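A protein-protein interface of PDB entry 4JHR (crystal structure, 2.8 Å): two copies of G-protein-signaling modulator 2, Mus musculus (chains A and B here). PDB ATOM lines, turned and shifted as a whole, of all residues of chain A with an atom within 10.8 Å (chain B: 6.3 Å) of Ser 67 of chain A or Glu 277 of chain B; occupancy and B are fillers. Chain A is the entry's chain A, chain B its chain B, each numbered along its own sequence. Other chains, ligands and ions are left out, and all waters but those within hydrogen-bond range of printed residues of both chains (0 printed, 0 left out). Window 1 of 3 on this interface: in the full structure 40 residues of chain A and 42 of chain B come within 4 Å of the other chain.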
ATOM      1  N   ASN A  26     -11.825  -0.977  14.888  1.00  0.00           N
ATOM      2  CA  ASN A  26     -10.711  -1.305  14.000  1.00  0.00           C
ATOM      3  C   ASN A  26     -11.047  -1.136  12.512  1.00  0.00           C
ATOM      4  O   ASN A  26     -10.327  -1.624  11.641  1.00  0.00           O
ATOM      5  CB  ASN A  26     -10.249  -2.738  14.258  1.00  0.00           C
ATOM      6  CG  ASN A  26      -8.879  -2.798  14.906  1.00  0.00           C
ATOM      7  OD1 ASN A  26      -8.098  -1.845  14.819  1.00  0.00           O
ATOM      8  ND2 ASN A  26      -8.573  -3.922  15.556  1.00  0.00           N
ATOM      9  N   PHE A  27     -12.130  -0.423  12.226  1.00  0.00           N
ATOM     10  CA  PHE A  27     -12.723  -0.481  10.899  1.00  0.00           C
ATOM     11  C   PHE A  27     -11.864   0.199   9.847  1.00  0.00           C
ATOM     12  O   PHE A  27     -12.040  -0.027   8.651  1.00  0.00           O
ATOM     13  CB  PHE A  27     -14.129   0.122  10.912  1.00  0.00           C
ATOM     14  CG  PHE A  27     -15.073  -0.531  11.903  1.00  0.00           C
ATOM     15  CD1 PHE A  27     -16.142  -1.294  11.459  1.00  0.00           C
ATOM     16  CD2 PHE A  27     -14.893  -0.376  13.279  1.00  0.00           C
ATOM     17  CE1 PHE A  27     -17.008  -1.888  12.364  1.00  0.00           C
ATOM     18  CE2 PHE A  27     -15.756  -0.962  14.183  1.00  0.00           C
ATOM     19  CZ  PHE A  27     -16.817  -1.716  13.726  1.00  0.00           C
ATOM     20  N   ASP A  28     -10.922   1.025  10.279  1.00  0.00           N
ATOM     21  CA  ASP A  28     -10.157   1.777   9.297  1.00  0.00           C
ATOM     22  C   ASP A  28      -8.906   1.057   8.841  1.00  0.00           C
ATOM     23  O   ASP A  28      -8.626   0.996   7.646  1.00  0.00           O
ATOM     24  CB  ASP A  28      -9.874   3.206   9.763  1.00  0.00           C
ATOM     25  CG  ASP A  28     -10.986   4.172   9.360  1.00  0.00           C
ATOM     26  OD1 ASP A  28     -12.183   3.785   9.438  1.00  0.00           O
ATOM     27  OD2 ASP A  28     -10.661   5.311   8.950  1.00  0.00           O
ATOM     28  N   GLU A  29      -8.154   0.500   9.779  1.00  0.00           N
ATOM     29  CA  GLU A  29      -7.030  -0.328   9.372  1.00  0.00           C
ATOM     30  C   GLU A  29      -7.532  -1.419   8.436  1.00  0.00           C
ATOM     31  O   GLU A  29      -6.946  -1.667   7.385  1.00  0.00           O
ATOM     32  CB  GLU A  29      -6.277  -0.909  10.573  1.00  0.00           C
ATOM     33  CG  GLU A  29      -5.259   0.080  11.161  1.00  0.00           C
ATOM     34  CD  GLU A  29      -4.287  -0.559  12.146  1.00  0.00           C
ATOM     35  OE1 GLU A  29      -4.671  -1.539  12.831  1.00  0.00           O
ATOM     36  OE2 GLU A  29      -3.134  -0.072  12.228  1.00  0.00           O
ATOM     37  N   ALA A  30      -8.662  -2.018   8.791  1.00  0.00           N
ATOM     38  CA  ALA A  30      -9.236  -3.094   7.996  1.00  0.00           C
ATOM     39  C   ALA A  30      -9.574  -2.685   6.586  1.00  0.00           C
ATOM     40  O   ALA A  30      -9.271  -3.420   5.653  1.00  0.00           O
ATOM     41  CB  ALA A  30     -10.442  -3.655   8.664  1.00  0.00           C
ATOM     42  N   ILE A  31     -10.211  -1.528   6.427  1.00  0.00           N
ATOM     43  CA  ILE A  31     -10.651  -1.100   5.100  1.00  0.00           C
ATOM     44  C   ILE A  31      -9.470  -0.877   4.141  1.00  0.00           C
ATOM     45  O   ILE A  31      -9.523  -1.237   2.973  1.00  0.00           O
ATOM     46  CB  ILE A  31     -11.590   0.144   5.152  1.00  0.00           C
ATOM     47  CG1 ILE A  31     -11.958   0.580   3.744  1.00  0.00           C
ATOM     48  CG2 ILE A  31     -10.934   1.317   5.846  1.00  0.00           C
ATOM     49  CD1 ILE A  31     -12.225   2.053   3.612  1.00  0.00           C
ATOM     50  N   ASN A  59     -18.090  -6.639   4.008  1.00  0.00           N
ATOM     51  CA  ASN A  59     -18.332  -7.103   5.368  1.00  0.00           C
ATOM     52  C   ASN A  59     -17.913  -6.089   6.426  1.00  0.00           C
ATOM     53  O   ASN A  59     -18.518  -6.006   7.503  1.00  0.00           O
ATOM     54  CB  ASN A  59     -17.653  -8.456   5.605  1.00  0.00           C
ATOM     55  CG  ASN A  59     -18.410  -9.581   4.987  1.00  0.00           C
ATOM     56  OD1 ASN A  59     -19.631  -9.521   4.901  1.00  0.00           O
ATOM     57  ND2 ASN A  59     -17.706 -10.611   4.531  1.00  0.00           N
ATOM     58  N   VAL A  60     -16.871  -5.324   6.122  1.00  0.00           N
ATOM     59  CA  VAL A  60     -16.374  -4.357   7.087  1.00  0.00           C
ATOM     60  C   VAL A  60     -17.342  -3.197   7.201  1.00  0.00           C
ATOM     61  O   VAL A  60     -17.777  -2.856   8.302  1.00  0.00           O
ATOM     62  CB  VAL A  60     -14.983  -3.852   6.717  1.00  0.00           C
ATOM     63  CG1 VAL A  60     -14.559  -2.752   7.675  1.00  0.00           C
ATOM     64  CG2 VAL A  60     -14.010  -5.014   6.752  1.00  0.00           C
ATOM     65  N   TYR A  61     -17.670  -2.611   6.049  1.00  0.00           N
ATOM     66  CA  TYR A  61     -18.689  -1.567   5.949  1.00  0.00           C
ATOM     67  C   TYR A  61     -19.980  -1.956   6.660  1.00  0.00           C
ATOM     68  O   TYR A  61     -20.454  -1.241   7.539  1.00  0.00           O
ATOM     69  CB  TYR A  61     -18.959  -1.235   4.483  1.00  0.00           C
ATOM     70  CG  TYR A  61     -17.975  -0.252   3.951  1.00  0.00           C
ATOM     71  CD1 TYR A  61     -17.632   0.881   4.683  1.00  0.00           C
ATOM     72  CD2 TYR A  61     -17.349  -0.460   2.735  1.00  0.00           C
ATOM     73  CE1 TYR A  61     -16.705   1.798   4.204  1.00  0.00           C
ATOM     74  CE2 TYR A  61     -16.419   0.448   2.243  1.00  0.00           C
ATOM     75  CZ  TYR A  61     -16.101   1.576   2.978  1.00  0.00           C
ATOM     76  OH  TYR A  61     -15.177   2.475   2.476  1.00  0.00           O
ATOM     77  N   HIS A  62     -20.531  -3.097   6.254  1.00  0.00           N
ATOM     78  CA  HIS A  62     -21.693  -3.714   6.876  1.00  0.00           C
ATOM     79  C   HIS A  62     -21.553  -3.626   8.386  1.00  0.00           C
ATOM     80  O   HIS A  62     -22.447  -3.152   9.058  1.00  0.00           O
ATOM     81  CB  HIS A  62     -21.754  -5.170   6.424  1.00  0.00           C
ATOM     82  CG  HIS A  62     -23.031  -5.873   6.760  1.00  0.00           C
ATOM     83  ND1 HIS A  62     -23.350  -7.105   6.235  1.00  0.00           N
ATOM     84  CD2 HIS A  62     -24.053  -5.537   7.578  1.00  0.00           C
ATOM     85  CE1 HIS A  62     -24.520  -7.494   6.706  1.00  0.00           C
ATOM     86  NE2 HIS A  62     -24.973  -6.556   7.515  1.00  0.00           N
ATOM     87  N   ALA A  63     -20.409  -4.029   8.917  1.00  0.00           N
ATOM     88  CA  ALA A  63     -20.220  -4.002  10.370  1.00  0.00           C
ATOM     89  C   ALA A  63     -20.017  -2.591  10.937  1.00  0.00           C
ATOM     90  O   ALA A  63     -20.382  -2.322  12.086  1.00  0.00           O
ATOM     91  CB  ALA A  63     -19.083  -4.919  10.788  1.00  0.00           C
ATOM     92  N   LYS A  64     -19.431  -1.701  10.137  1.00  0.00           N
ATOM     93  CA  LYS A  64     -19.332  -0.287  10.499  1.00  0.00           C
ATOM     94  C   LYS A  64     -20.727   0.316  10.564  1.00  0.00           C
ATOM     95  O   LYS A  64     -21.061   1.061  11.487  1.00  0.00           O
ATOM     96  CB  LYS A  64     -18.466   0.487   9.493  1.00  0.00           C
ATOM     97  N   GLY A  65     -21.543  -0.029   9.580  1.00  0.00           N
ATOM     98  CA  GLY A  65     -22.900   0.477   9.502  1.00  0.00           C
ATOM     99  C   GLY A  65     -23.745   0.234  10.739  1.00  0.00           C
ATOM    100  O   GLY A  65     -24.617   1.046  11.049  1.00  0.00           O
ATOM    101  N   LYS A  66     -23.502  -0.866  11.456  1.00  0.00           N
ATOM    102  CA  LYS A  66     -24.236  -1.119  12.698  1.00  0.00           C
ATOM    103  C   LYS A  66     -23.416  -0.844  13.958  1.00  0.00           C
ATOM    104  O   LYS A  66     -23.650  -1.465  14.993  1.00  0.00           O
ATOM    105  CB  LYS A  66     -24.807  -2.543  12.725  1.00  0.00           C
ATOM    106  N   SER A  67     -22.470   0.092  13.879  1.00  0.00           N
ATOM    107  CA  SER A  67     -21.652   0.471  15.043  1.00  0.00           C
ATOM    108  C   SER A  67     -21.036   1.860  14.913  1.00  0.00           C
ATOM    109  O   SER A  67     -20.317   2.310  15.806  1.00  0.00           O
ATOM    110  CB  SER A  67     -20.544  -0.561  15.305  1.00  0.00           C
ATOM    111  OG  SER A  67     -21.070  -1.773  15.821  1.00  0.00           O
ATOM    112  N   GLU A  81     -26.850   9.478  10.804  1.00  0.00           N
ATOM    113  CA  GLU A  81     -27.248   8.865   9.538  1.00  0.00           C
ATOM    114  C   GLU A  81     -26.222   9.078   8.405  1.00  0.00           C
ATOM    115  O   GLU A  81     -26.590   9.188   7.224  1.00  0.00           O
ATOM    116  CB  GLU A  81     -28.639   9.341   9.120  1.00  0.00           C
ATOM    117  N   ASP A  82     -24.944   9.150   8.786  1.00  0.00           N
ATOM    118  CA  ASP A  82     -23.823   8.979   7.858  1.00  0.00           C
ATOM    119  C   ASP A  82     -23.449   7.502   7.922  1.00  0.00           C
ATOM    120  O   ASP A  82     -22.542   7.038   7.238  1.00  0.00           O
ATOM    121  CB  ASP A  82     -22.628   9.855   8.249  1.00  0.00           C
ATOM    122  N   VAL A  83     -24.154   6.796   8.803  1.00  0.00           N
ATOM    123  CA  VAL A  83     -24.241   5.340   8.816  1.00  0.00           C
ATOM    124  C   VAL A  83     -24.810   4.822   7.491  1.00  0.00           C
ATOM    125  O   VAL A  83     -24.348   3.810   6.953  1.00  0.00           O
ATOM    126  CB  VAL A  83     -25.169   4.882   9.968  1.00  0.00           C
ATOM    127  CG1 VAL A  83     -25.928   3.604   9.603  1.00  0.00           C
ATOM    128  CG2 VAL A  83     -24.384   4.728  11.275  1.00  0.00           C
ATOM    129  N   ARG A  84     -25.809   5.527   6.960  1.00  0.00           N
ATOM    130  CA  ARG A  84     -26.386   5.185   5.661  1.00  0.00           C
ATOM    131  C   ARG A  84     -25.308   5.157   4.580  1.00  0.00           C
ATOM    132  O   ARG A  84     -25.438   4.455   3.571  1.00  0.00           O
ATOM    133  CB  ARG A  84     -27.495   6.166   5.273  1.00  0.00           C
ATOM    134  N   ALA A  86     -22.107   4.079   5.211  1.00  0.00           N
ATOM    135  CA  ALA A  86     -21.433   2.795   5.422  1.00  0.00           C
ATOM    136  C   ALA A  86     -22.257   1.654   4.854  1.00  0.00           C
ATOM    137  O   ALA A  86     -21.738   0.746   4.191  1.00  0.00           O
ATOM    138  CB  ALA A  86     -21.207   2.557   6.889  1.00  0.00           C
ATOM    139  N   LEU A  87     -23.554   1.710   5.116  1.00  0.00           N
ATOM    140  CA  LEU A  87     -24.444   0.645   4.702  1.00  0.00           C
ATOM    141  C   LEU A  87     -24.694   0.623   3.194  1.00  0.00           C
ATOM    142  O   LEU A  87     -24.744  -0.437   2.595  1.00  0.00           O
ATOM    143  CB  LEU A  87     -25.747   0.732   5.493  1.00  0.00           C
ATOM    144  CG  LEU A  87     -26.037  -0.405   6.486  1.00  0.00           C
ATOM    145  CD1 LEU A  87     -24.779  -1.016   7.042  1.00  0.00           C
ATOM    146  CD2 LEU A  87     -26.893   0.077   7.619  1.00  0.00           C
ATOM    147  N   LEU A 123     -31.415  -3.485   7.088  1.00  0.00           N
ATOM    148  CA  LEU A 123     -30.977  -2.458   8.011  1.00  0.00           C
ATOM    149  C   LEU A 123     -31.256  -1.059   7.467  1.00  0.00           C
ATOM    150  O   LEU A 123     -31.325  -0.084   8.231  1.00  0.00           O
ATOM    151  CB  LEU A 123     -29.489  -2.602   8.266  1.00  0.00           C
ATOM    152  CG  LEU A 123     -29.039  -3.795   9.096  1.00  0.00           C
ATOM    153  CD1 LEU A 123     -27.505  -3.911   9.086  1.00  0.00           C
ATOM    154  CD2 LEU A 123     -29.555  -3.641  10.493  1.00  0.00           C
ATOM    155  N   PRO A 275     -26.022  -9.023  21.316  1.00  0.00           N
ATOM    156  CA  PRO A 275     -26.134  -7.696  21.946  1.00  0.00           C
ATOM    157  C   PRO A 275     -27.540  -7.068  21.995  1.00  0.00           C
ATOM    158  O   PRO A 275     -27.848  -6.189  21.179  1.00  0.00           O
ATOM    159  CB  PRO A 275     -25.199  -6.821  21.087  1.00  0.00           C
ATOM    160  CG  PRO A 275     -24.709  -7.709  19.937  1.00  0.00           C
ATOM    161  CD  PRO A 275     -25.597  -8.914  19.910  1.00  0.00           C
ATOM    162  N   GLU A 277     -29.974  -4.670  22.355  1.00  0.00           N
ATOM    163  CA  GLU A 277     -30.056  -3.222  22.458  1.00  0.00           C
ATOM    164  C   GLU A 277     -31.466  -2.706  22.190  1.00  0.00           C
ATOM    165  O   GLU A 277     -31.633  -1.635  21.581  1.00  0.00           O
ATOM    166  CB  GLU A 277     -29.092  -2.566  21.478  1.00  0.00           C
ATOM    167  CG  GLU A 277     -27.692  -2.390  22.018  1.00  0.00           C
ATOM    168  CD  GLU A 277     -26.671  -2.150  20.924  1.00  0.00           C
ATOM    169  OE1 GLU A 277     -27.060  -2.125  19.729  1.00  0.00           O
ATOM    170  OE2 GLU A 277     -25.478  -1.992  21.269  1.00  0.00           O
ATOM    171  N   LYS B  66     -21.028   2.820  22.640  1.00  0.00           N
ATOM    172  CA  LYS B  66     -20.396   1.793  21.799  1.00  0.00           C
ATOM    173  C   LYS B  66     -21.237   1.312  20.611  1.00  0.00           C
ATOM    174  O   LYS B  66     -21.108   0.170  20.187  1.00  0.00           O
ATOM    175  CB  LYS B  66     -19.913   0.598  22.624  1.00  0.00           C
ATOM    176  CG  LYS B  66     -20.522   0.488  23.981  1.00  0.00           C
ATOM    177  CD  LYS B  66     -19.925  -0.680  24.725  1.00  0.00           C
ATOM    178  CE  LYS B  66     -20.474  -2.031  24.288  1.00  0.00           C
ATOM    179  NZ  LYS B  66     -19.723  -3.120  25.002  1.00  0.00           N
ATOM    180  N   SER B  67     -22.075   2.191  20.064  1.00  0.00           N
ATOM    181  CA  SER B  67     -22.884   1.859  18.891  1.00  0.00           C
ATOM    182  C   SER B  67     -23.401   3.072  18.114  1.00  0.00           C
ATOM    183  O   SER B  67     -24.078   2.913  17.091  1.00  0.00           O
ATOM    184  CB  SER B  67     -24.076   0.988  19.288  1.00  0.00           C
ATOM    185  OG  SER B  67     -23.654  -0.292  19.711  1.00  0.00           O
ATOM    186  N   PHE B  68     -23.107   4.277  18.589  1.00  0.00           N
ATOM    187  CA  PHE B  68     -23.601   5.473  17.913  1.00  0.00           C
ATOM    188  C   PHE B  68     -22.891   6.726  18.393  1.00  0.00           C
ATOM    189  O   PHE B  68     -23.526   7.758  18.588  1.00  0.00           O
ATOM    190  CB  PHE B  68     -25.120   5.625  18.105  1.00  0.00           C
ATOM    191  N   VAL B  83     -19.552  10.396  20.079  1.00  0.00           N
ATOM    192  CA  VAL B  83     -19.614   9.234  20.954  1.00  0.00           C
ATOM    193  C   VAL B  83     -19.047   9.597  22.334  1.00  0.00           C
ATOM    194  O   VAL B  83     -19.616   9.236  23.363  1.00  0.00           O
ATOM    195  CB  VAL B  83     -18.779   8.067  20.347  1.00  0.00           C
ATOM    196  CG1 VAL B  83     -18.132   7.210  21.432  1.00  0.00           C
ATOM    197  CG2 VAL B  83     -19.614   7.222  19.389  1.00  0.00           C
ATOM    198  N   PRO B 275     -19.697  -9.857  19.850  1.00  0.00           N
ATOM    199  CA  PRO B 275     -19.493  -9.229  18.536  1.00  0.00           C
ATOM    200  C   PRO B 275     -18.037  -8.908  18.178  1.00  0.00           C
ATOM    201  O   PRO B 275     -17.623  -7.751  18.323  1.00  0.00           O
ATOM    202  CB  PRO B 275     -20.317  -7.930  18.630  1.00  0.00           C
ATOM    203  CG  PRO B 275     -20.830  -7.860  20.077  1.00  0.00           C
ATOM    204  CD  PRO B 275     -20.050  -8.863  20.873  1.00  0.00           C
ATOM    205  N   ASP B 276     -17.299  -9.909  17.690  1.00  0.00           N
ATOM    206  CA  ASP B 276     -15.911  -9.743  17.239  1.00  0.00           C
ATOM    207  C   ASP B 276     -15.776  -8.705  16.120  1.00  0.00           C
ATOM    208  O   ASP B 276     -16.054  -8.988  14.948  1.00  0.00           O
ATOM    209  CB  ASP B 276     -15.311 -11.082  16.781  1.00  0.00           C
ATOM    210  N   GLU B 277     -15.335  -7.507  16.495  1.00  0.00           N
ATOM    211  CA  GLU B 277     -15.145  -6.434  15.540  1.00  0.00           C
ATOM    212  C   GLU B 277     -13.689  -6.009  15.470  1.00  0.00           C
ATOM    213  O   GLU B 277     -13.379  -4.820  15.290  1.00  0.00           O
ATOM    214  CB  GLU B 277     -16.016  -5.236  15.917  1.00  0.00           C
ATOM    215  CG  GLU B 277     -17.424  -5.273  15.339  1.00  0.00           C
ATOM    216  CD  GLU B 277     -18.377  -4.293  16.034  1.00  0.00           C
ATOM    217  OE1 GLU B 277     -17.946  -3.573  16.970  1.00  0.00           O
ATOM    218  OE2 GLU B 277     -19.566  -4.250  15.642  1.00  0.00           O
ATOM    219  N   ASP B 278     -12.778  -6.960  15.616  1.00  0.00           N
ATOM    220  CA  ASP B 278     -11.374  -6.578  15.527  1.00  0.00           C
ATOM    221  C   ASP B 278     -10.712  -6.990  14.223  1.00  0.00           C
ATOM    222  O   ASP B 278      -9.520  -6.807  14.057  1.00  0.00           O
ATOM    223  CB  ASP B 278     -10.555  -6.959  16.775  1.00  0.00           C
ATOM    224  CG  ASP B 278     -10.682  -8.412  17.143  1.00  0.00           C
ATOM    225  OD1 ASP B 278     -10.548  -9.270  16.237  1.00  0.00           O
ATOM    226  OD2 ASP B 278     -10.900  -8.687  18.349  1.00  0.00           O
ATOM    227  N   PHE B 279     -11.508  -7.499  13.288  1.00  0.00           N
ATOM    228  CA  PHE B 279     -11.057  -7.745  11.916  1.00  0.00           C
ATOM    229  C   PHE B 279      -9.714  -8.472  11.857  1.00  0.00           C
ATOM    230  O   PHE B 279      -8.820  -8.141  11.069  1.00  0.00           O
ATOM    231  CB  PHE B 279     -11.058  -6.426  11.139  1.00  0.00           C
ATOM    232  CG  PHE B 279     -12.385  -5.734  11.194  1.00  0.00           C
ATOM    233  CD1 PHE B 279     -13.415  -6.116  10.350  1.00  0.00           C
ATOM    234  CD2 PHE B 279     -12.635  -4.768  12.141  1.00  0.00           C
ATOM    235  CE1 PHE B 279     -14.648  -5.516  10.421  1.00  0.00           C
ATOM    236  CE2 PHE B 279     -13.871  -4.173  12.216  1.00  0.00           C
ATOM    237  CZ  PHE B 279     -14.879  -4.548  11.352  1.00  0.00           C
ATOM    238  N   PHE B 280      -9.620  -9.486  12.709  1.00  0.00           N
ATOM    239  CA  PHE B 280      -8.399 -10.225  12.937  1.00  0.00           C
ATOM    240  C   PHE B 280      -7.854 -10.857  11.661  1.00  0.00           C
ATOM    241  O   PHE B 280      -6.677 -10.688  11.322  1.00  0.00           O
ATOM    242  CB  PHE B 280      -8.638 -11.308  13.994  1.00  0.00           C
ATOM    243  CG  PHE B 280      -7.387 -11.992  14.450  1.00  0.00           C
ATOM    244  CD1 PHE B 280      -6.667 -11.503  15.525  1.00  0.00           C
ATOM    245  CD2 PHE B 280      -6.917 -13.111  13.802  1.00  0.00           C
ATOM    246  CE1 PHE B 280      -5.503 -12.134  15.947  1.00  0.00           C
ATOM    247  CE2 PHE B 280      -5.743 -13.741  14.220  1.00  0.00           C
ATOM    248  CZ  PHE B 280      -5.045 -13.260  15.286  1.00  0.00           C
ATOM    249  N   ALA B 302     -19.722 -13.043  12.638  1.00  0.00           N
ATOM    250  CA  ALA B 302     -18.559 -12.403  13.248  1.00  0.00           C
ATOM    251  C   ALA B 302     -18.639 -12.440  14.770  1.00  0.00           C
ATOM    252  O   ALA B 302     -18.771 -11.399  15.414  1.00  0.00           O
ATOM    253  CB  ALA B 302     -18.402 -10.970  12.745  1.00  0.00           C
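O of Asp 278 of chain B is in hydrogen-bond range of ND2 of Asn 26 of chain A (3.4 Å).
The side-chain hydroxyl of Ser 67 of chain A lies within hydrogen-bond range of the side-chain carboxylate of Glu 277 of chain B (2.9 Å).
The side-chain carboxylate (OE2) of Glu 277 of chain A lies within hydrogen-bond range of the side-chain hydroxyl (OG) of Ser 67 of chain B, at 2.9 Å.
Among the printed residues, merely in contact across the chains: Phe 27 of chain A with Phe 279 of chain B (3.5 Å), Val 60 of chain A with Phe 279 of chain B (3.8 Å), Ala 30 of chain A with Phe 279 of chain B (3.8 Å), Asn 26 of chain A with Phe 279 of chain B (3.8 Å), Phe 27 of chain A with Glu 277 of chain B (3.8 Å), Pro 275 of chain A with Pro 275 of chain B (3.9 Å), Ser 67 of chain A with Ser 67 of chain B (3.9 Å) and Asn 26 of chain A with Glu 277 of chain B (3.9 Å).
Of the printed residues of chain B, Asn 26 of chain A touches Glu 277 (3.9 Å), Asp 278 (3.4 Å) and Phe 279 (3.8 Å).
Of the printed residues of chain B, Phe 27 of chain A touches Glu 277 and Phe 279.
Of the printed residues of chain B, Val 60 of chain A touches Phe 279 (3.8 Å).
Leu 87 of chain A touches none of the printed residues of chain B.
Of the printed residues of chain B, Glu 277 of chain A touches Ser 67.
Of the printed residues of chain A, Ser 67 of chain B touches Ser 67 (3.9 Å) and Glu 277 (2.9 Å).
Pro 275 of chain B touches just one residue of chain A: Pro 275.
No residue of chain A comes within 4 Å of Asp 276 of chain B.
Glu 277 of chain B touches just these residues of chain A: Asn 26, Phe 27 and Ser 67.
Of chain A, only Asn 26 comes within 4 Å of Asp 278 of chain B.
The nearest residue of chain B that does not touch Ser 67 of chain A is Phe 68 of chain B (4.4 Å).
The nearest residue of chain A that does not touch Glu 277 of chain B is Ala 63 of chain A (4.1 Å).
The nearest printed residue of chain B that does not touch Glu 277 of chain A is Lys 66 of chain B (5.0 Å).
Printed residues of chain A that touch a printed residue of chain B: Asn 26, Phe 27, Ala 30, Val 60, Ser 67, Pro 275 and Glu 277.
Hydrophobic or aromatic side chains of chain A within 4 Å of the printed part of chain B: Phe 27, Ala 30, Val 60 and Pro 275.
Along chain A the printed residues that touch a printed residue of chain B span positions 26 to 277.
Of the 11 printed residues of chain B, 5 touch a printed residue of chain A.
Printed residues of chain B that touch a printed residue of chain A: Ser 67, Pro 275, Glu 277, Asp 278 and Phe 279.
Hydrophobic or aromatic side chains of chain B within 4 Å of the printed part of chain A: Pro 275 and Phe 279.
Among the printed residues, 11 pairs touch across the chains.
Among the printed residues, no Asp or Glu carboxylate lies within 4 Å of a Lys or Arg side-chain nitrogen of the other chain.
Ser 67 of chain B touches its own counterpart, Ser 67 of chain A.
Ser 67 of chain A touches Glu 277 of chain B, and with the chains exchanged Glu 277 of chain A touches Ser 67 of chain B.
Pro 275 of chain B touches its own counterpart, Pro 275 of chain A.
Of the 11 pairs that touch across the chains among the printed residues, 4 have their exchanged pair printed and touching as well.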
